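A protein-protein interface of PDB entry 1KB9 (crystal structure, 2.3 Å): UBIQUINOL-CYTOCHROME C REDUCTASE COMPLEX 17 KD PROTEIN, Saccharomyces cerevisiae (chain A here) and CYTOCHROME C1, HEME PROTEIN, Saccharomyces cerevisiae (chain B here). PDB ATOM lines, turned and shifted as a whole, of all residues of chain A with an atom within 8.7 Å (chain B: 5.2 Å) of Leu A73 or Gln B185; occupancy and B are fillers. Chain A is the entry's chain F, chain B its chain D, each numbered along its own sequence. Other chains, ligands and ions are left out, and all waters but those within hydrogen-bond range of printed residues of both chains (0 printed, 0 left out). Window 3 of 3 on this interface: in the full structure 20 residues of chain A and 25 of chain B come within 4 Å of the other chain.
Hydrophobic or aromatic side chains of chain B within 4 Å of the printed part of chain A: Phe B131. Along chain B the printed residues that touch a printed residue of chain A span positions 31 to 188. Printed residues of chain A that touch a printed residue of chain B: Asp A3, Gln A4, Leu A5, Leu A69, Phe A70, Leu A73 and Lys A74. Among the printed residues, 14 pairs touch across the chains. Among the printed residues, no Asp or Glu carboxylate lies within 4 Å of a Lys or Arg side-chain nitrogen of the other chain.
The side-chain hydroxyl (OG) of Ser B184 sits at hydrogen-bond distance from the side-chain carboxylate (OD1) of Asp A3 (3.0 Å). The backbone carbonyl oxygen (O) of Lys A74 sits at hydrogen-bond distance from the side-chain amide nitrogen (NE2) of Gln B185 (3.0 Å). The side-chain hydroxyl (OG1) of Thr B182 lies within hydrogen-bond range of the side-chain amide nitrogen (NE2) of Gln A4 (2.6 Å). The side-chain amide nitrogen (NE2) of Gln A4 sits at hydrogen-bond distance from the side-chain hydroxyl (OG) of Ser B184 (3.2 Å). The side-chain carboxylate of Asp A3 is in hydrogen-bond range of the side-chain hydroxyl of Thr B183 (3.4 Å). NZ of Lys B188 lies within hydrogen-bond range of O of Lys A74 (3.2 Å). The guanidinium group (NH2) of Arg B31 is in hydrogen-bond range of the backbone carbonyl oxygen (O) of Lys A74, 3.3 Å away.
Thr B182 touches Asp A3. CB of Leu A5 touches CB of Ser B184, at 3.97 Å. CD2 of Leu A69 touches CZ of Phe B131 (3.7 Å). CE2 of Phe A70 touches CG of Lys B188, 3.5 Å away. CD2 of Leu A73 touches OG of Ser B184, at 3.5 Å. Gln B185 touches Leu A73. Lys B188 touches Leu A73.
Arg A68 touches none of the printed residues of chain B. Printed residues of chain B within 4 Å of Phe A70: Lys B188. Of chain B, only Ser B184, Gln B185 and Lys B188 come within 4 Å of Leu A73. Printed residues of chain B within 4 Å of Lys A74: Arg B31 (3.3 Å), Gln B185 (3.0 Å) and Lys B188 (3.2 Å). Of the printed residues of chain A, Thr B183 touches Asp A3. Of chain A, only Asp A3, Gln A4, Leu A5 and Leu A73 come within 4 Å of Ser B184. Of chain A, only Leu A73 and Lys A74 come within 4 Å of Gln B185. Of the printed residues of chain A, Lys B188 touches Phe A70, Leu A73 and Lys A74. The nearest residue of chain A that does not touch Gln B185 is Gln A4 (4.8 Å).
The side-chain hydroxyl of Thr B182 lies close to the backbone NH of Gln B185 (3.3 Å). N of Leu A5 sits close to OD2 of Asp A3, at 3.4 Å. The side-chain carboxylate (OD2) of Asp B189 lies within hydrogen-bond range of the side-chain amide nitrogen (NE2) of Gln B185 (3.3 Å). The guanidinium group (NH2) of Arg B31 lies close to the side-chain amide nitrogen (NE2) of Gln B185, at 2.8 Å. The guanidinium group (NH2) of Arg B31 is in salt-bridge range of the side-chain carboxylate (OD1) of Asp B189 (2.8 Å).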
ATOM      1  N   THR A   2      13.477 -23.530 -29.048  1.00  0.00           N
ATOM      2  CA  THR A   2      12.357 -22.744 -29.560  1.00  0.00           C
ATOM      3  C   THR A   2      12.185 -21.474 -28.713  1.00  0.00           C
ATOM      4  O   THR A   2      12.374 -21.506 -27.489  1.00  0.00           O
ATOM      5  CB  THR A   2      11.047 -23.573 -29.554  1.00  0.00           C
ATOM      6  OG1 THR A   2       9.968 -22.782 -30.070  1.00  0.00           O
ATOM      7  CG2 THR A   2      10.707 -24.040 -28.139  1.00  0.00           C
ATOM      8  N   ASP A   3      11.837 -20.363 -29.366  1.00  0.00           N
ATOM      9  CA  ASP A   3      11.654 -19.087 -28.670  1.00  0.00           C
ATOM     10  C   ASP A   3      10.702 -19.184 -27.481  1.00  0.00           C
ATOM     11  O   ASP A   3       9.576 -19.662 -27.611  1.00  0.00           O
ATOM     12  CB  ASP A   3      11.177 -17.993 -29.626  1.00  0.00           C
ATOM     13  CG  ASP A   3      11.001 -16.652 -28.927  1.00  0.00           C
ATOM     14  OD1 ASP A   3      11.964 -16.200 -28.273  1.00  0.00           O
ATOM     15  OD2 ASP A   3       9.899 -16.066 -29.014  1.00  0.00           O
ATOM     16  N   GLN A   4      11.164 -18.680 -26.338  1.00  0.00           N
ATOM     17  CA  GLN A   4      10.418 -18.704 -25.086  1.00  0.00           C
ATOM     18  C   GLN A   4       9.113 -17.913 -25.103  1.00  0.00           C
ATOM     19  O   GLN A   4       8.134 -18.307 -24.465  1.00  0.00           O
ATOM     20  CB  GLN A   4      11.307 -18.218 -23.941  1.00  0.00           C
ATOM     21  CG  GLN A   4      12.555 -19.065 -23.688  1.00  0.00           C
ATOM     22  CD  GLN A   4      13.772 -18.632 -24.497  1.00  0.00           C
ATOM     23  OE1 GLN A   4      14.909 -18.897 -24.105  1.00  0.00           O
ATOM     24  NE2 GLN A   4      13.543 -17.964 -25.621  1.00  0.00           N
ATOM     25  N   LEU A   5       9.104 -16.791 -25.817  1.00  0.00           N
ATOM     26  CA  LEU A   5       7.914 -15.955 -25.912  1.00  0.00           C
ATOM     27  C   LEU A   5       6.857 -16.632 -26.789  1.00  0.00           C
ATOM     28  O   LEU A   5       5.686 -16.710 -26.408  1.00  0.00           O
ATOM     29  CB  LEU A   5       8.280 -14.571 -26.460  1.00  0.00           C
ATOM     30  CG  LEU A   5       7.192 -13.496 -26.527  1.00  0.00           C
ATOM     31  CD1 LEU A   5       6.553 -13.284 -25.169  1.00  0.00           C
ATOM     32  CD2 LEU A   5       7.800 -12.207 -27.026  1.00  0.00           C
ATOM     33  N   LEU A   8       5.112 -19.400 -24.771  1.00  0.00           N
ATOM     34  CA  LEU A   8       4.110 -18.895 -23.831  1.00  0.00           C
ATOM     35  C   LEU A   8       2.880 -18.311 -24.525  1.00  0.00           C
ATOM     36  O   LEU A   8       1.771 -18.384 -23.996  1.00  0.00           O
ATOM     37  CB  LEU A   8       4.726 -17.864 -22.882  1.00  0.00           C
ATOM     38  CG  LEU A   8       5.587 -18.408 -21.741  1.00  0.00           C
ATOM     39  CD1 LEU A   8       6.183 -17.262 -20.945  1.00  0.00           C
ATOM     40  CD2 LEU A   8       4.737 -19.282 -20.841  1.00  0.00           C
ATOM     41  N   ARG A  68       5.886 -13.696 -16.771  1.00  0.00           N
ATOM     42  CA  ARG A  68       6.537 -15.003 -16.755  1.00  0.00           C
ATOM     43  C   ARG A  68       7.731 -15.182 -17.683  1.00  0.00           C
ATOM     44  O   ARG A  68       8.639 -15.954 -17.378  1.00  0.00           O
ATOM     45  CB  ARG A  68       5.508 -16.097 -17.071  1.00  0.00           C
ATOM     46  CG  ARG A  68       4.617 -16.494 -15.907  1.00  0.00           C
ATOM     47  CD  ARG A  68       3.612 -17.566 -16.322  1.00  0.00           C
ATOM     48  NE  ARG A  68       2.390 -16.987 -16.872  1.00  0.00           N
ATOM     49  CZ  ARG A  68       1.247 -16.879 -16.199  1.00  0.00           C
ATOM     50  NH1 ARG A  68       0.184 -16.329 -16.775  1.00  0.00           N
ATOM     51  NH2 ARG A  68       1.159 -17.326 -14.950  1.00  0.00           N
ATOM     52  N   LEU A  69       7.731 -14.475 -18.808  1.00  0.00           N
ATOM     53  CA  LEU A  69       8.799 -14.599 -19.798  1.00  0.00           C
ATOM     54  C   LEU A  69      10.248 -14.542 -19.298  1.00  0.00           C
ATOM     55  O   LEU A  69      11.086 -15.337 -19.738  1.00  0.00           O
ATOM     56  CB  LEU A  69       8.599 -13.581 -20.925  1.00  0.00           C
ATOM     57  CG  LEU A  69       9.661 -13.593 -22.029  1.00  0.00           C
ATOM     58  CD1 LEU A  69       9.732 -14.973 -22.672  1.00  0.00           C
ATOM     59  CD2 LEU A  69       9.351 -12.533 -23.068  1.00  0.00           C
ATOM     60  N   PHE A  70      10.542 -13.630 -18.376  1.00  0.00           N
ATOM     61  CA  PHE A  70      11.907 -13.481 -17.884  1.00  0.00           C
ATOM     62  C   PHE A  70      12.451 -14.573 -16.959  1.00  0.00           C
ATOM     63  O   PHE A  70      13.668 -14.749 -16.855  1.00  0.00           O
ATOM     64  CB  PHE A  70      12.132 -12.069 -17.327  1.00  0.00           C
ATOM     65  CG  PHE A  70      12.277 -11.019 -18.401  1.00  0.00           C
ATOM     66  CD1 PHE A  70      11.549 -11.106 -19.584  1.00  0.00           C
ATOM     67  CD2 PHE A  70      13.166  -9.966 -18.249  1.00  0.00           C
ATOM     68  CE1 PHE A  70      11.706 -10.163 -20.598  1.00  0.00           C
ATOM     69  CE2 PHE A  70      13.329  -9.017 -19.255  1.00  0.00           C
ATOM     70  CZ  PHE A  70      12.598  -9.117 -20.434  1.00  0.00           C
ATOM     71  N   ASP A  71      11.567 -15.312 -16.295  1.00  0.00           N
ATOM     72  CA  ASP A  71      12.018 -16.409 -15.444  1.00  0.00           C
ATOM     73  C   ASP A  71      12.560 -17.525 -16.343  1.00  0.00           C
ATOM     74  O   ASP A  71      13.320 -18.384 -15.897  1.00  0.00           O
ATOM     75  CB  ASP A  71      10.881 -16.942 -14.570  1.00  0.00           C
ATOM     76  CG  ASP A  71      10.635 -16.084 -13.344  1.00  0.00           C
ATOM     77  OD1 ASP A  71       9.458 -15.745 -13.086  1.00  0.00           O
ATOM     78  OD2 ASP A  71      11.611 -15.755 -12.629  1.00  0.00           O
ATOM     79  N   LYS A  72      12.174 -17.492 -17.616  1.00  0.00           N
ATOM     80  CA  LYS A  72      12.627 -18.478 -18.586  1.00  0.00           C
ATOM     81  C   LYS A  72      13.841 -17.993 -19.374  1.00  0.00           C
ATOM     82  O   LYS A  72      14.445 -18.754 -20.126  1.00  0.00           O
ATOM     83  CB  LYS A  72      11.488 -18.857 -19.541  1.00  0.00           C
ATOM     84  CG  LYS A  72      10.334 -19.589 -18.864  1.00  0.00           C
ATOM     85  CD  LYS A  72      10.834 -20.821 -18.098  1.00  0.00           C
ATOM     86  CE  LYS A  72       9.701 -21.556 -17.391  1.00  0.00           C
ATOM     87  NZ  LYS A  72       8.676 -22.067 -18.351  1.00  0.00           N
ATOM     88  N   LEU A  73      14.187 -16.721 -19.209  1.00  0.00           N
ATOM     89  CA  LEU A  73      15.333 -16.144 -19.900  1.00  0.00           C
ATOM     90  C   LEU A  73      16.540 -16.053 -18.980  1.00  0.00           C
ATOM     91  O   LEU A  73      16.423 -16.182 -17.760  1.00  0.00           O
ATOM     92  CB  LEU A  73      14.996 -14.756 -20.451  1.00  0.00           C
ATOM     93  CG  LEU A  73      13.981 -14.667 -21.591  1.00  0.00           C
ATOM     94  CD1 LEU A  73      13.802 -13.215 -22.004  1.00  0.00           C
ATOM     95  CD2 LEU A  73      14.458 -15.485 -22.772  1.00  0.00           C
ATOM     96  N   LYS A  74      17.707 -15.858 -19.583  1.00  0.00           N
ATOM     97  CA  LYS A  74      18.948 -15.739 -18.837  1.00  0.00           C
ATOM     98  C   LYS A  74      19.339 -14.263 -18.747  1.00  0.00           C
ATOM     99  O   LYS A  74      19.243 -13.559 -19.778  1.00  0.00           O
ATOM    100  CB  LYS A  74      20.049 -16.572 -19.517  1.00  0.00           C
ATOM    101  CG  LYS A  74      21.469 -16.374 -18.969  1.00  0.00           C
ATOM    102  CD  LYS A  74      21.592 -16.705 -17.476  1.00  0.00           C
ATOM    103  CE  LYS A  74      23.024 -16.479 -16.962  1.00  0.00           C
ATOM    104  NZ  LYS A  74      23.522 -15.072 -17.137  1.00  0.00           N
ATOM    105  N   ARG B  31      26.268  -9.180 -23.772  1.00  0.00           N
ATOM    106  CA  ARG B  31      25.582  -9.858 -24.870  1.00  0.00           C
ATOM    107  C   ARG B  31      24.861  -8.861 -25.774  1.00  0.00           C
ATOM    108  O   ARG B  31      24.909  -8.982 -27.003  1.00  0.00           O
ATOM    109  CB  ARG B  31      24.571 -10.870 -24.326  1.00  0.00           C
ATOM    110  CG  ARG B  31      25.156 -12.224 -23.942  1.00  0.00           C
ATOM    111  CD  ARG B  31      24.074 -13.150 -23.403  1.00  0.00           C
ATOM    112  NE  ARG B  31      24.108 -13.246 -21.948  1.00  0.00           N
ATOM    113  CZ  ARG B  31      23.042 -13.138 -21.163  1.00  0.00           C
ATOM    114  NH1 ARG B  31      23.170 -13.250 -19.848  1.00  0.00           N
ATOM    115  NH2 ARG B  31      21.856 -12.886 -21.685  1.00  0.00           N
ATOM    116  N   PHE B 131      11.565  -3.664 -26.203  1.00  0.00           N
ATOM    117  CA  PHE B 131      11.499  -5.108 -26.237  1.00  0.00           C
ATOM    118  C   PHE B 131      10.255  -5.567 -26.998  1.00  0.00           C
ATOM    119  O   PHE B 131      10.351  -6.329 -27.962  1.00  0.00           O
ATOM    120  CB  PHE B 131      11.485  -5.678 -24.822  1.00  0.00           C
ATOM    121  CG  PHE B 131      11.446  -7.177 -24.784  1.00  0.00           C
ATOM    122  CD1 PHE B 131      12.623  -7.915 -24.816  1.00  0.00           C
ATOM    123  CD2 PHE B 131      10.233  -7.853 -24.743  1.00  0.00           C
ATOM    124  CE1 PHE B 131      12.593  -9.304 -24.811  1.00  0.00           C
ATOM    125  CE2 PHE B 131      10.192  -9.237 -24.738  1.00  0.00           C
ATOM    126  CZ  PHE B 131      11.379  -9.968 -24.772  1.00  0.00           C
ATOM    127  N   TYR B 175      26.142 -16.530 -29.259  1.00  0.00           N
ATOM    128  CA  TYR B 175      26.586 -15.948 -27.999  1.00  0.00           C
ATOM    129  C   TYR B 175      27.891 -16.528 -27.495  1.00  0.00           C
ATOM    130  O   TYR B 175      28.036 -17.741 -27.338  1.00  0.00           O
ATOM    131  CB  TYR B 175      25.511 -16.060 -26.918  1.00  0.00           C
ATOM    132  CG  TYR B 175      24.465 -14.968 -26.980  1.00  0.00           C
ATOM    133  CD1 TYR B 175      23.159 -15.205 -26.548  1.00  0.00           C
ATOM    134  CD2 TYR B 175      24.779 -13.697 -27.473  1.00  0.00           C
ATOM    135  CE1 TYR B 175      22.193 -14.209 -26.609  1.00  0.00           C
ATOM    136  CE2 TYR B 175      23.821 -12.691 -27.536  1.00  0.00           C
ATOM    137  CZ  TYR B 175      22.530 -12.954 -27.104  1.00  0.00           C
ATOM    138  OH  TYR B 175      21.570 -11.973 -27.175  1.00  0.00           O
ATOM    139  N   THR B 179      24.976 -18.932 -24.250  1.00  0.00           N
ATOM    140  CA  THR B 179      23.534 -18.737 -24.066  1.00  0.00           C
ATOM    141  C   THR B 179      22.738 -18.950 -25.361  1.00  0.00           C
ATOM    142  O   THR B 179      23.185 -18.565 -26.448  1.00  0.00           O
ATOM    143  CB  THR B 179      23.250 -17.315 -23.496  1.00  0.00           C
ATOM    144  OG1 THR B 179      23.926 -17.165 -22.241  1.00  0.00           O
ATOM    145  CG2 THR B 179      21.753 -17.086 -23.289  1.00  0.00           C
ATOM    146  N   PRO B 180      21.580 -19.636 -25.267  1.00  0.00           N
ATOM    147  CA  PRO B 180      20.728 -19.898 -26.434  1.00  0.00           C
ATOM    148  C   PRO B 180      20.211 -18.569 -26.992  1.00  0.00           C
ATOM    149  O   PRO B 180      19.417 -17.875 -26.350  1.00  0.00           O
ATOM    150  CB  PRO B 180      19.580 -20.729 -25.846  1.00  0.00           C
ATOM    151  CG  PRO B 180      20.196 -21.397 -24.662  1.00  0.00           C
ATOM    152  CD  PRO B 180      21.047 -20.304 -24.066  1.00  0.00           C
ATOM    153  N   ALA B 181      20.658 -18.230 -28.192  1.00  0.00           N
ATOM    154  CA  ALA B 181      20.273 -16.988 -28.828  1.00  0.00           C
ATOM    155  C   ALA B 181      18.881 -16.934 -29.448  1.00  0.00           C
ATOM    156  O   ALA B 181      18.742 -16.729 -30.656  1.00  0.00           O
ATOM    157  CB  ALA B 181      21.322 -16.585 -29.849  1.00  0.00           C
ATOM    158  N   THR B 182      17.847 -17.094 -28.623  1.00  0.00           N
ATOM    159  CA  THR B 182      16.470 -17.004 -29.115  1.00  0.00           C
ATOM    160  C   THR B 182      16.140 -15.525 -29.377  1.00  0.00           C
ATOM    161  O   THR B 182      16.848 -14.637 -28.889  1.00  0.00           O
ATOM    162  CB  THR B 182      15.468 -17.579 -28.109  1.00  0.00           C
ATOM    163  OG1 THR B 182      15.575 -16.874 -26.867  1.00  0.00           O
ATOM    164  CG2 THR B 182      15.740 -19.058 -27.874  1.00  0.00           C
ATOM    165  N   THR B 183      15.073 -15.254 -30.128  1.00  0.00           N
ATOM    166  CA  THR B 183      14.723 -13.865 -30.438  1.00  0.00           C
ATOM    167  C   THR B 183      14.400 -13.046 -29.194  1.00  0.00           C
ATOM    168  O   THR B 183      14.859 -11.912 -29.066  1.00  0.00           O
ATOM    169  CB  THR B 183      13.548 -13.736 -31.439  1.00  0.00           C
ATOM    170  OG1 THR B 183      12.303 -13.814 -30.738  1.00  0.00           O
ATOM    171  CG2 THR B 183      13.603 -14.830 -32.486  1.00  0.00           C
ATOM    172  N   SER B 184      13.640 -13.635 -28.274  1.00  0.00           N
ATOM    173  CA  SER B 184      13.261 -12.940 -27.048  1.00  0.00           C
ATOM    174  C   SER B 184      14.468 -12.726 -26.141  1.00  0.00           C
ATOM    175  O   SER B 184      14.512 -11.764 -25.375  1.00  0.00           O
ATOM    176  CB  SER B 184      12.153 -13.695 -26.304  1.00  0.00           C
ATOM    177  OG  SER B 184      12.655 -14.856 -25.669  1.00  0.00           O
ATOM    178  N   GLN B 185      15.443 -13.625 -26.233  1.00  0.00           N
ATOM    179  CA  GLN B 185      16.663 -13.525 -25.434  1.00  0.00           C
ATOM    180  C   GLN B 185      17.536 -12.399 -25.974  1.00  0.00           C
ATOM    181  O   GLN B 185      18.108 -11.627 -25.208  1.00  0.00           O
ATOM    182  CB  GLN B 185      17.438 -14.842 -25.481  1.00  0.00           C
ATOM    183  CG  GLN B 185      18.797 -14.796 -24.820  1.00  0.00           C
ATOM    184  CD  GLN B 185      18.728 -14.790 -23.311  1.00  0.00           C
ATOM    185  OE1 GLN B 185      18.002 -15.577 -22.699  1.00  0.00           O
ATOM    186  NE2 GLN B 185      19.513 -13.919 -22.694  1.00  0.00           N
ATOM    187  N   MET B 186      17.647 -12.326 -27.297  1.00  0.00           N
ATOM    188  CA  MET B 186      18.446 -11.297 -27.940  1.00  0.00           C
ATOM    189  C   MET B 186      17.820  -9.926 -27.737  1.00  0.00           C
ATOM    190  O   MET B 186      18.525  -8.944 -27.536  1.00  0.00           O
ATOM    191  CB  MET B 186      18.599 -11.583 -29.431  1.00  0.00           C
ATOM    192  CG  MET B 186      19.448 -12.804 -29.736  1.00  0.00           C
ATOM    193  SD  MET B 186      19.714 -12.984 -31.490  1.00  0.00           S
ATOM    194  CE  MET B 186      18.101 -13.566 -31.988  1.00  0.00           C
ATOM    195  N   ALA B 187      16.491  -9.869 -27.789  1.00  0.00           N
ATOM    196  CA  ALA B 187      15.772  -8.622 -27.594  1.00  0.00           C
ATOM    197  C   ALA B 187      15.996  -8.151 -26.161  1.00  0.00           C
ATOM    198  O   ALA B 187      16.283  -6.982 -25.925  1.00  0.00           O
ATOM    199  CB  ALA B 187      14.298  -8.822 -27.861  1.00  0.00           C
ATOM    200  N   LYS B 188      15.911  -9.084 -25.217  1.00  0.00           N
ATOM    201  CA  LYS B 188      16.112  -8.787 -23.804  1.00  0.00           C
ATOM    202  C   LYS B 188      17.510  -8.214 -23.576  1.00  0.00           C
ATOM    203  O   LYS B 188      17.681  -7.289 -22.790  1.00  0.00           O
ATOM    204  CB  LYS B 188      15.900 -10.060 -22.975  1.00  0.00           C
ATOM    205  CG  LYS B 188      15.940  -9.902 -21.457  1.00  0.00           C
ATOM    206  CD  LYS B 188      17.333 -10.136 -20.888  1.00  0.00           C
ATOM    207  CE  LYS B 188      17.286 -10.497 -19.409  1.00  0.00           C
ATOM    208  NZ  LYS B 188      18.657 -10.543 -18.806  1.00  0.00           N
ATOM    209  N   ASP B 189      18.492  -8.734 -24.309  1.00  0.00           N
ATOM    210  CA  ASP B 189      19.873  -8.286 -24.181  1.00  0.00           C
ATOM    211  C   ASP B 189      20.185  -6.917 -24.798  1.00  0.00           C
ATOM    212  O   ASP B 189      20.820  -6.101 -24.139  1.00  0.00           O
ATOM    213  CB  ASP B 189      20.845  -9.348 -24.730  1.00  0.00           C
ATOM    214  CG  ASP B 189      20.831 -10.650 -23.923  1.00  0.00           C
ATOM    215  OD1 ASP B 189      20.456 -10.641 -22.729  1.00  0.00           O
ATOM    216  OD2 ASP B 189      21.208 -11.698 -24.490  1.00  0.00           O
